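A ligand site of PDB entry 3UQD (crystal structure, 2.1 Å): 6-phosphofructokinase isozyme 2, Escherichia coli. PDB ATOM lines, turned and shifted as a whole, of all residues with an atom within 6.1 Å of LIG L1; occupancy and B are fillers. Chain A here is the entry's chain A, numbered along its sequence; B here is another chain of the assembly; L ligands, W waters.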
ATOM      1  N   ALA A  10     -19.891  26.039  29.505  1.00  0.00           N
ATOM      2  CA  ALA A  10     -19.615  24.785  30.184  1.00  0.00           C
ATOM      3  C   ALA A  10     -18.288  24.177  29.744  1.00  0.00           C
ATOM      4  O   ALA A  10     -18.259  23.315  28.871  1.00  0.00           O
ATOM      5  CB  ALA A  10     -20.753  23.777  29.947  1.00  0.00           C
ATOM      6  N   SER A  12     -14.549  22.077  30.419  1.00  0.00           N
ATOM      7  CA  SER A  12     -14.323  20.730  30.929  1.00  0.00           C
ATOM      8  C   SER A  12     -12.836  20.410  31.083  1.00  0.00           C
ATOM      9  O   SER A  12     -12.023  20.799  30.248  1.00  0.00           O
ATOM     10  CB  SER A  12     -14.982  19.708  29.999  1.00  0.00           C
ATOM     11  OG  SER A  12     -14.775  18.384  30.464  1.00  0.00           O
ATOM     12  N   ASP A  14     -10.860  17.363  30.598  1.00  0.00           N
ATOM     13  CA  ASP A  14     -10.983  16.018  30.052  1.00  0.00           C
ATOM     14  C   ASP A  14      -9.831  15.108  30.467  1.00  0.00           C
ATOM     15  O   ASP A  14      -8.667  15.435  30.247  1.00  0.00           O
ATOM     16  CB  ASP A  14     -11.103  16.049  28.520  1.00  0.00           C
ATOM     17  CG  ASP A  14     -12.386  16.692  28.056  1.00  0.00           C
ATOM     18  OD1 ASP A  14     -13.242  16.990  28.904  1.00  0.00           O
ATOM     19  OD2 ASP A  14     -12.534  16.899  26.834  1.00  0.00           O
ATOM     20  N   PRO A  37      -7.638  20.103  27.584  1.00  0.00           N
ATOM     21  CA  PRO A  37      -8.761  21.044  27.711  1.00  0.00           C
ATOM     22  C   PRO A  37     -10.023  20.553  27.001  1.00  0.00           C
ATOM     23  O   PRO A  37      -9.921  19.941  25.939  1.00  0.00           O
ATOM     24  CB  PRO A  37      -8.233  22.320  27.040  1.00  0.00           C
ATOM     25  CG  PRO A  37      -6.749  22.183  27.065  1.00  0.00           C
ATOM     26  CD  PRO A  37      -6.498  20.714  26.873  1.00  0.00           C
ATOM     27  N   GLY A  38     -11.178  20.820  27.594  1.00  0.00           N
ATOM     28  CA  GLY A  38     -12.447  20.367  27.030  1.00  0.00           C
ATOM     29  C   GLY A  38     -13.494  21.466  27.028  1.00  0.00           C
ATOM     30  O   GLY A  38     -13.396  22.441  27.772  1.00  0.00           O
ATOM     31  N   GLY A  39     -14.515  21.300  26.195  1.00  0.00           N
ATOM     32  CA  GLY A  39     -15.527  22.332  26.013  1.00  0.00           C
ATOM     33  C   GLY A  39     -15.505  22.845  24.583  1.00  0.00           C
ATOM     34  O   GLY A  39     -14.453  22.924  23.965  1.00  0.00           O
ATOM     35  N   GLY A  40     -16.682  23.187  24.053  1.00  0.00           N
ATOM     36  CA  GLY A  40     -16.839  23.500  22.641  1.00  0.00           C
ATOM     37  C   GLY A  40     -16.063  24.717  22.198  1.00  0.00           C
ATOM     38  O   GLY A  40     -15.293  24.648  21.246  1.00  0.00           O
ATOM     39  N   ASN A  43     -12.279  24.185  22.462  1.00  0.00           N
ATOM     40  CA  ASN A  43     -11.753  23.391  21.360  1.00  0.00           C
ATOM     41  C   ASN A  43     -11.718  24.158  20.040  1.00  0.00           C
ATOM     42  O   ASN A  43     -10.816  23.954  19.227  1.00  0.00           O
ATOM     43  CB  ASN A  43     -12.537  22.091  21.201  1.00  0.00           C
ATOM     44  CG  ASN A  43     -12.237  21.100  22.304  1.00  0.00           C
ATOM     45  OD1 ASN A  43     -11.167  21.146  22.917  1.00  0.00           O
ATOM     46  ND2 ASN A  43     -13.178  20.207  22.582  1.00  0.00           N
ATOM     47  N   ARG A  90     -16.035  20.740  35.839  1.00  0.00           N
ATOM     48  CA  ARG A  90     -16.332  19.326  35.671  1.00  0.00           C
ATOM     49  C   ARG A  90     -15.176  18.569  35.033  1.00  0.00           C
ATOM     50  O   ARG A  90     -14.298  19.154  34.396  1.00  0.00           O
ATOM     51  CB  ARG A  90     -17.562  19.144  34.797  1.00  0.00           C
ATOM     52  CG  ARG A  90     -17.368  19.676  33.389  1.00  0.00           C
ATOM     53  CD  ARG A  90     -18.463  19.205  32.456  1.00  0.00           C
ATOM     54  NE  ARG A  90     -18.463  19.992  31.218  1.00  0.00           N
ATOM     55  CZ  ARG A  90     -19.134  19.670  30.128  1.00  0.00           C
ATOM     56  NH1 ARG A  90     -19.860  18.568  30.101  1.00  0.00           N
ATOM     57  NH2 ARG A  90     -19.065  20.448  29.058  1.00  0.00           N
ATOM     58  N   ASN A  92     -14.530  15.198  32.564  1.00  0.00           N
ATOM     59  CA  ASN A  92     -15.038  14.116  31.721  1.00  0.00           C
ATOM     60  C   ASN A  92     -14.029  12.972  31.584  1.00  0.00           C
ATOM     61  O   ASN A  92     -12.832  13.174  31.792  1.00  0.00           O
ATOM     62  CB  ASN A  92     -15.417  14.658  30.335  1.00  0.00           C
ATOM     63  CG  ASN A  92     -16.553  15.681  30.402  1.00  0.00           C
ATOM     64  OD1 ASN A  92     -17.345  15.683  31.354  1.00  0.00           O
ATOM     65  ND2 ASN A  92     -16.643  16.540  29.402  1.00  0.00           N
ATOM     66  N   ARG A 105     -16.878   7.795  25.726  1.00  0.00           N
ATOM     67  CA  ARG A 105     -16.825   9.186  26.181  1.00  0.00           C
ATOM     68  C   ARG A 105     -17.917   9.509  27.185  1.00  0.00           C
ATOM     69  O   ARG A 105     -19.068   9.745  26.805  1.00  0.00           O
ATOM     70  CB  ARG A 105     -16.941  10.118  24.987  1.00  0.00           C
ATOM     71  CG  ARG A 105     -15.948   9.827  23.885  1.00  0.00           C
ATOM     72  CD  ARG A 105     -16.395  10.436  22.566  1.00  0.00           C
ATOM     73  NE  ARG A 105     -16.492  11.890  22.642  1.00  0.00           N
ATOM     74  CZ  ARG A 105     -16.887  12.660  21.630  1.00  0.00           C
ATOM     75  NH1 ARG A 105     -17.237  12.112  20.474  1.00  0.00           N
ATOM     76  NH2 ARG A 105     -16.942  13.977  21.770  1.00  0.00           N
ATOM     77  N   VAL A 107     -19.650  11.944  29.476  1.00  0.00           N
ATOM     78  CA  VAL A 107     -19.796  13.395  29.568  1.00  0.00           C
ATOM     79  C   VAL A 107     -20.660  13.853  30.743  1.00  0.00           C
ATOM     80  O   VAL A 107     -21.875  13.666  30.748  1.00  0.00           O
ATOM     81  CB  VAL A 107     -20.383  13.960  28.267  1.00  0.00           C
ATOM     82  CG1 VAL A 107     -20.455  15.485  28.332  1.00  0.00           C
ATOM     83  CG2 VAL A 107     -19.546  13.507  27.078  1.00  0.00           C
ATOM     84  N   MET A 108     -20.009  14.467  31.727  1.00  0.00           N
ATOM     85  CA  MET A 108     -20.676  14.988  32.924  1.00  0.00           C
ATOM     86  C   MET A 108     -21.355  16.333  32.642  1.00  0.00           C
ATOM     87  O   MET A 108     -21.019  16.992  31.659  1.00  0.00           O
ATOM     88  CB  MET A 108     -19.656  15.152  34.048  1.00  0.00           C
ATOM     89  CG  MET A 108     -18.760  13.948  34.238  1.00  0.00           C
ATOM     90  SD  MET A 108     -19.690  12.505  34.759  1.00  0.00           S
ATOM     91  CE  MET A 108     -18.788  11.223  33.904  1.00  0.00           C
ATOM     92  N   GLY A 110     -22.107  20.334  32.961  1.00  0.00           N
ATOM     93  CA  GLY A 110     -21.248  21.471  33.224  1.00  0.00           C
ATOM     94  C   GLY A 110     -21.380  21.942  34.657  1.00  0.00           C
ATOM     95  O   GLY A 110     -22.360  21.622  35.332  1.00  0.00           O
ATOM     96  N   GLY A 138     -20.854  24.836  22.691  1.00  0.00           N
ATOM     97  CA  GLY A 138     -20.923  23.951  23.838  1.00  0.00           C
ATOM     98  C   GLY A 138     -22.289  23.955  24.476  1.00  0.00           C
ATOM     99  O   GLY A 138     -23.157  24.747  24.105  1.00  0.00           O
ATOM    100  N   SER A 139     -22.489  23.077  25.450  1.00  0.00           N
ATOM    101  CA  SER A 139     -23.779  22.949  26.117  1.00  0.00           C
ATOM    102  C   SER A 139     -24.021  24.080  27.121  1.00  0.00           C
ATOM    103  O   SER A 139     -23.175  24.964  27.299  1.00  0.00           O
ATOM    104  CB  SER A 139     -23.892  21.589  26.815  1.00  0.00           C
ATOM    105  OG  SER A 139     -22.858  21.412  27.766  1.00  0.00           O
ATOM    106  N   LEU A 140     -25.182  24.044  27.778  1.00  0.00           N
ATOM    107  CA  LEU A 140     -25.524  25.020  28.801  1.00  0.00           C
ATOM    108  C   LEU A 140     -25.442  24.382  30.184  1.00  0.00           C
ATOM    109  O   LEU A 140     -26.025  23.335  30.413  1.00  0.00           O
ATOM    110  CB  LEU A 140     -26.941  25.549  28.599  1.00  0.00           C
ATOM    111  CG  LEU A 140     -27.103  26.897  27.889  1.00  0.00           C
ATOM    112  CD1 LEU A 140     -28.559  27.340  27.942  1.00  0.00           C
ATOM    113  CD2 LEU A 140     -26.205  27.936  28.521  1.00  0.00           C
ATOM    114  N   VAL A 252     -13.951  12.200  16.709  1.00  0.00           N
ATOM    115  CA  VAL A 252     -14.151  13.185  17.781  1.00  0.00           C
ATOM    116  C   VAL A 252     -13.232  14.389  17.568  1.00  0.00           C
ATOM    117  O   VAL A 252     -12.061  14.243  17.224  1.00  0.00           O
ATOM    118  CB  VAL A 252     -13.989  12.574  19.200  1.00  0.00           C
ATOM    119  CG1 VAL A 252     -13.265  11.255  19.150  1.00  0.00           C
ATOM    120  CG2 VAL A 252     -13.303  13.564  20.157  1.00  0.00           C
ATOM    121  N   GLY A 253     -13.797  15.585  17.738  1.00  0.00           N
ATOM    122  CA  GLY A 253     -13.068  16.812  17.474  1.00  0.00           C
ATOM    123  C   GLY A 253     -13.369  17.380  16.099  1.00  0.00           C
ATOM    124  O   GLY A 253     -13.044  18.539  15.816  1.00  0.00           O
ATOM    125  N   ASP A 256     -15.757  20.680  16.220  1.00  0.00           N
ATOM    126  CA  ASP A 256     -15.106  21.899  16.709  1.00  0.00           C
ATOM    127  C   ASP A 256     -13.962  22.365  15.794  1.00  0.00           C
ATOM    128  O   ASP A 256     -13.673  23.563  15.704  1.00  0.00           O
ATOM    129  CB  ASP A 256     -14.580  21.684  18.133  1.00  0.00           C
ATOM    130  CG  ASP A 256     -15.704  21.564  19.162  1.00  0.00           C
ATOM    131  OD1 ASP A 256     -16.740  22.239  19.002  1.00  0.00           O
ATOM    132  OD2 ASP A 256     -15.539  20.807  20.147  1.00  0.00           O
ATOM    133  N   LYS B  27     -21.091  10.588  22.446  1.00  0.00           N
ATOM    134  CA  LYS B  27     -21.075  11.156  23.789  1.00  0.00           C
ATOM    135  C   LYS B  27     -22.127  10.482  24.669  1.00  0.00           C
ATOM    136  O   LYS B  27     -23.308  10.483  24.331  1.00  0.00           O
ATOM    137  CB  LYS B  27     -21.359  12.664  23.765  1.00  0.00           C
ATOM    138  CG  LYS B  27     -20.284  13.520  23.120  1.00  0.00           C
ATOM    139  CD  LYS B  27     -20.622  15.005  23.275  1.00  0.00           C
ATOM    140  CE  LYS B  27     -19.598  15.884  22.583  1.00  0.00           C
ATOM    141  NZ  LYS B  27     -19.894  17.330  22.729  1.00  0.00           N
ATOM    142  N   ARG B  29     -24.056  10.959  27.797  1.00  0.00           N
ATOM    143  CA  ARG B  29     -24.484  11.889  28.840  1.00  0.00           C
ATOM    144  C   ARG B  29     -24.623  11.179  30.181  1.00  0.00           C
ATOM    145  O   ARG B  29     -25.323  10.171  30.302  1.00  0.00           O
ATOM    146  CB  ARG B  29     -25.812  12.541  28.461  1.00  0.00           C
ATOM    147  CG  ARG B  29     -25.749  13.414  27.221  1.00  0.00           C
ATOM    148  CD  ARG B  29     -24.978  14.678  27.489  1.00  0.00           C
ATOM    149  NE  ARG B  29     -25.045  15.610  26.365  1.00  0.00           N
ATOM    150  CZ  ARG B  29     -24.443  16.791  26.344  1.00  0.00           C
ATOM    151  NH1 ARG B  29     -23.726  17.191  27.392  1.00  0.00           N
ATOM    152  NH2 ARG B  29     -24.553  17.578  25.285  1.00  0.00           N
HETATM  153  O1  LIG L   1     -15.928  17.593  21.074  1.00  0.00           O
HETATM  154  C1  LIG L   1     -15.671  17.025  22.334  1.00  0.00           C
HETATM  155  C2  LIG L   1     -16.044  17.997  23.441  1.00  0.00           C
HETATM  156  O2  LIG L   1     -16.101  19.343  22.913  1.00  0.00           O
HETATM  157  C3  LIG L   1     -15.058  17.957  24.603  1.00  0.00           C
HETATM  158  O3  LIG L   1     -14.272  19.118  24.615  1.00  0.00           O
HETATM  159  C4  LIG L   1     -15.911  17.898  25.859  1.00  0.00           C
HETATM  160  O4  LIG L   1     -15.530  16.809  26.674  1.00  0.00           O
HETATM  161  C5  LIG L   1     -17.337  17.735  25.381  1.00  0.00           C
HETATM  162  O5  LIG L   1     -17.312  17.656  23.971  1.00  0.00           O
HETATM  163  C6  LIG L   1     -18.150  18.962  25.762  1.00  0.00           C
HETATM  164  O6  LIG L   1     -19.231  18.662  26.611  1.00  0.00           O
HETATM  165  P1  LIG L   1     -20.728  19.092  26.204  1.00  0.00           P
HETATM  166  O7  LIG L   1     -20.665  20.463  25.549  1.00  0.00           O
HETATM  167  O8  LIG L   1     -21.555  19.209  27.457  1.00  0.00           O
HETATM  168  O9  LIG L   1     -21.338  18.091  25.250  1.00  0.00           O
HETATM  169  P1  LG2 L   2     -19.094  16.522  16.516  1.00  0.00           P
HETATM  170  O1  LG2 L   2     -17.606  16.260  16.787  1.00  0.00           O
HETATM  171  O2  LG2 L   2     -19.450  17.651  17.421  1.00  0.00           O
HETATM  172  O3  LG2 L   2     -19.934  15.301  16.787  1.00  0.00           O
HETATM  173  P2  LG2 L   2     -20.571  17.252  14.290  1.00  0.00           P
HETATM  174  O4  LG2 L   2     -21.197  18.531  14.899  1.00  0.00           O
HETATM  175  O5  LG2 L   2     -21.566  16.045  14.447  1.00  0.00           O
HETATM  176  O6  LG2 L   2     -19.200  16.905  15.021  1.00  0.00           O
HETATM  177  P3  LG2 L   2     -19.911  16.319  11.772  1.00  0.00           P
HETATM  178  O7  LG2 L   2     -20.094  14.969  12.421  1.00  0.00           O
HETATM  179  O8  LG2 L   2     -20.747  16.425  10.501  1.00  0.00           O
HETATM  180  O9  LG2 L   2     -20.231  17.442  12.757  1.00  0.00           O
HETATM  181  O10 LG2 L   2     -18.347  16.447  11.412  1.00  0.00           O
HETATM  182  C1  LG2 L   2     -17.891  17.615  10.835  1.00  0.00           C
HETATM  183  C2  LG2 L   2     -16.966  17.507   9.718  1.00  0.00           C
HETATM  184  O11 LG2 L   2     -15.955  16.538  10.074  1.00  0.00           O
HETATM  185  C3  LG2 L   2     -17.601  16.909   8.541  1.00  0.00           C
HETATM  186  O12 LG2 L   2     -18.242  17.855   7.787  1.00  0.00           O
HETATM  187  C4  LG2 L   2     -16.450  16.340   7.831  1.00  0.00           C
HETATM  188  O13 LG2 L   2     -15.733  17.339   7.240  1.00  0.00           O
HETATM  189  C5  LG2 L   2     -15.659  15.756   8.945  1.00  0.00           C
HETATM  190  N1  LG2 L   2     -15.994  14.356   9.187  1.00  0.00           N
HETATM  191  C6  LG2 L   2     -16.828  13.921  10.156  1.00  0.00           C
HETATM  192  N2  LG2 L   2     -16.898  12.576  10.045  1.00  0.00           N
HETATM  193  C7  LG2 L   2     -16.130  12.170   9.017  1.00  0.00           C
HETATM  194  C8  LG2 L   2     -15.813  10.917   8.471  1.00  0.00           C
HETATM  195  N3  LG2 L   2     -16.408   9.664   9.051  1.00  0.00           N
HETATM  196  N4  LG2 L   2     -14.976  10.856   7.424  1.00  0.00           N
HETATM  197  C9  LG2 L   2     -14.433  11.971   6.900  1.00  0.00           C
HETATM  198  N5  LG2 L   2     -14.705  13.171   7.409  1.00  0.00           N
HETATM  199  C10 LG2 L   2     -15.534  13.310   8.457  1.00  0.00           C
HETATM  200  O   HOH W   1     -12.913  15.735  23.217  1.00  0.00           O
HETATM  201  O   HOH W   2     -18.803  18.044  20.181  1.00  0.00           O
HETATM  202  O   HOH W   3     -15.801  18.452  18.035  1.00  0.00           O
HETATM  203  O   HOH W   4     -16.328  15.431  19.214  1.00  0.00           O
HETATM  204  O   HOH W   5     -19.014  22.867  26.222  1.00  0.00           O
HETATM  205  O   HOH W   6     -19.309  20.879  23.175  1.00  0.00           O
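NZ of Lys 27 of chain B lies within salt-bridge range of O9 of LIG L1.
N of Ser 139 lies within hydrogen-bond range of O7 of LIG L1 (3.2 Å).
The side-chain amide nitrogen of Asn 43 sits at hydrogen-bond distance from an oxygen (O3) of LIG L1.
The guanidinium group of Arg 29 of chain B is in salt-bridge range of an oxygen (O8) of LIG L1.
The backbone NH (N) of Gly 39 is in hydrogen-bond range of an oxygen (O3) of LIG L1 (2.7 Å).
The guanidinium group of Arg 90 is in salt-bridge range of an oxygen (O8) of LIG L1.
An oxygen (O8) of LIG L1 lies within hydrogen-bond range of the side-chain hydroxyl (OG) of Ser 139 (2.6 Å).
The side-chain carboxylate (OD2) of Asp 14 is in hydrogen-bond range of an oxygen (O4) of LIG L1 (3.0 Å).
The side-chain carboxylate (OD2) of Asp 256 lies within hydrogen-bond range of an oxygen (O2) of LIG L1 (3.2 Å).
The side-chain amide nitrogen (ND2) of Asn 92 lies within hydrogen-bond range of an oxygen (O4) of LIG L1, 3.0 Å away.
Gly 38 touches LIG L1 (CA to O3, 3.3 Å).
Arg 105 touches LIG L1 (NH2 to C1, 3.4 Å).
Val 107 touches LIG L1 (CG1 to O6, 3.8 Å).
Gly 138 touches LIG L1 (CA to O7, 3.9 Å).
Hydrophobic or aromatic side chains that line LIG L1: Val 107.
Of the 22 residues printed, 13 come within 4 Å of LIG L1.
Water W4 lies within hydrogen-bond range of O1 of LG2 L2, O1 of LIG L1, N of Gly 253 and NH2 of Arg 105.
Water W5 lies within hydrogen-bond range of O of Ala 10 (2.8 Å), O7 of LIG L1 (3.0 Å) and N of Gly 40 (3.2 Å).
Water W2 lies within hydrogen-bond range of the side-chain amino group of Lys 27 of chain B (2.9 Å) and an oxygen (O1) of LIG L1 (3.0 Å).
Water W3 lies within hydrogen-bond range of N of Asp 256 (2.9 Å), O1 of LG2 L2 (3.1 Å) and O1 of LIG L1 (3.2 Å).
OD1 of Asn 43 lies close to O of Pro 37, at 3.5 Å.
The side-chain amide nitrogen of Asn 43 lies close to the side-chain carboxylate of Asp 256.
The guanidinium group (NH2) of Arg 90 sits at hydrogen-bond distance from the backbone carbonyl oxygen (O) of Ala 10 (3.0 Å).
The side-chain amide nitrogen (ND2) of Asn 43 lies within hydrogen-bond range of the backbone carbonyl oxygen (O) of Gly 39 (3.3 Å).
The side-chain hydroxyl (OG) of Ser 12 sits at hydrogen-bond distance from the side-chain carboxylate (OD1) of Asp 14 (2.6 Å).
The backbone NH (N) of Met 108 lies within hydrogen-bond range of the side-chain amide oxygen (OD1) of Asn 92, 3.0 Å away.
ND2 of Asn 92 lies within hydrogen-bond range of OG of Ser 12 (2.8 Å).
The backbone NH of Gly 38 sits at hydrogen-bond distance from the backbone carbonyl oxygen of Ser 12, at 2.8 Å.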
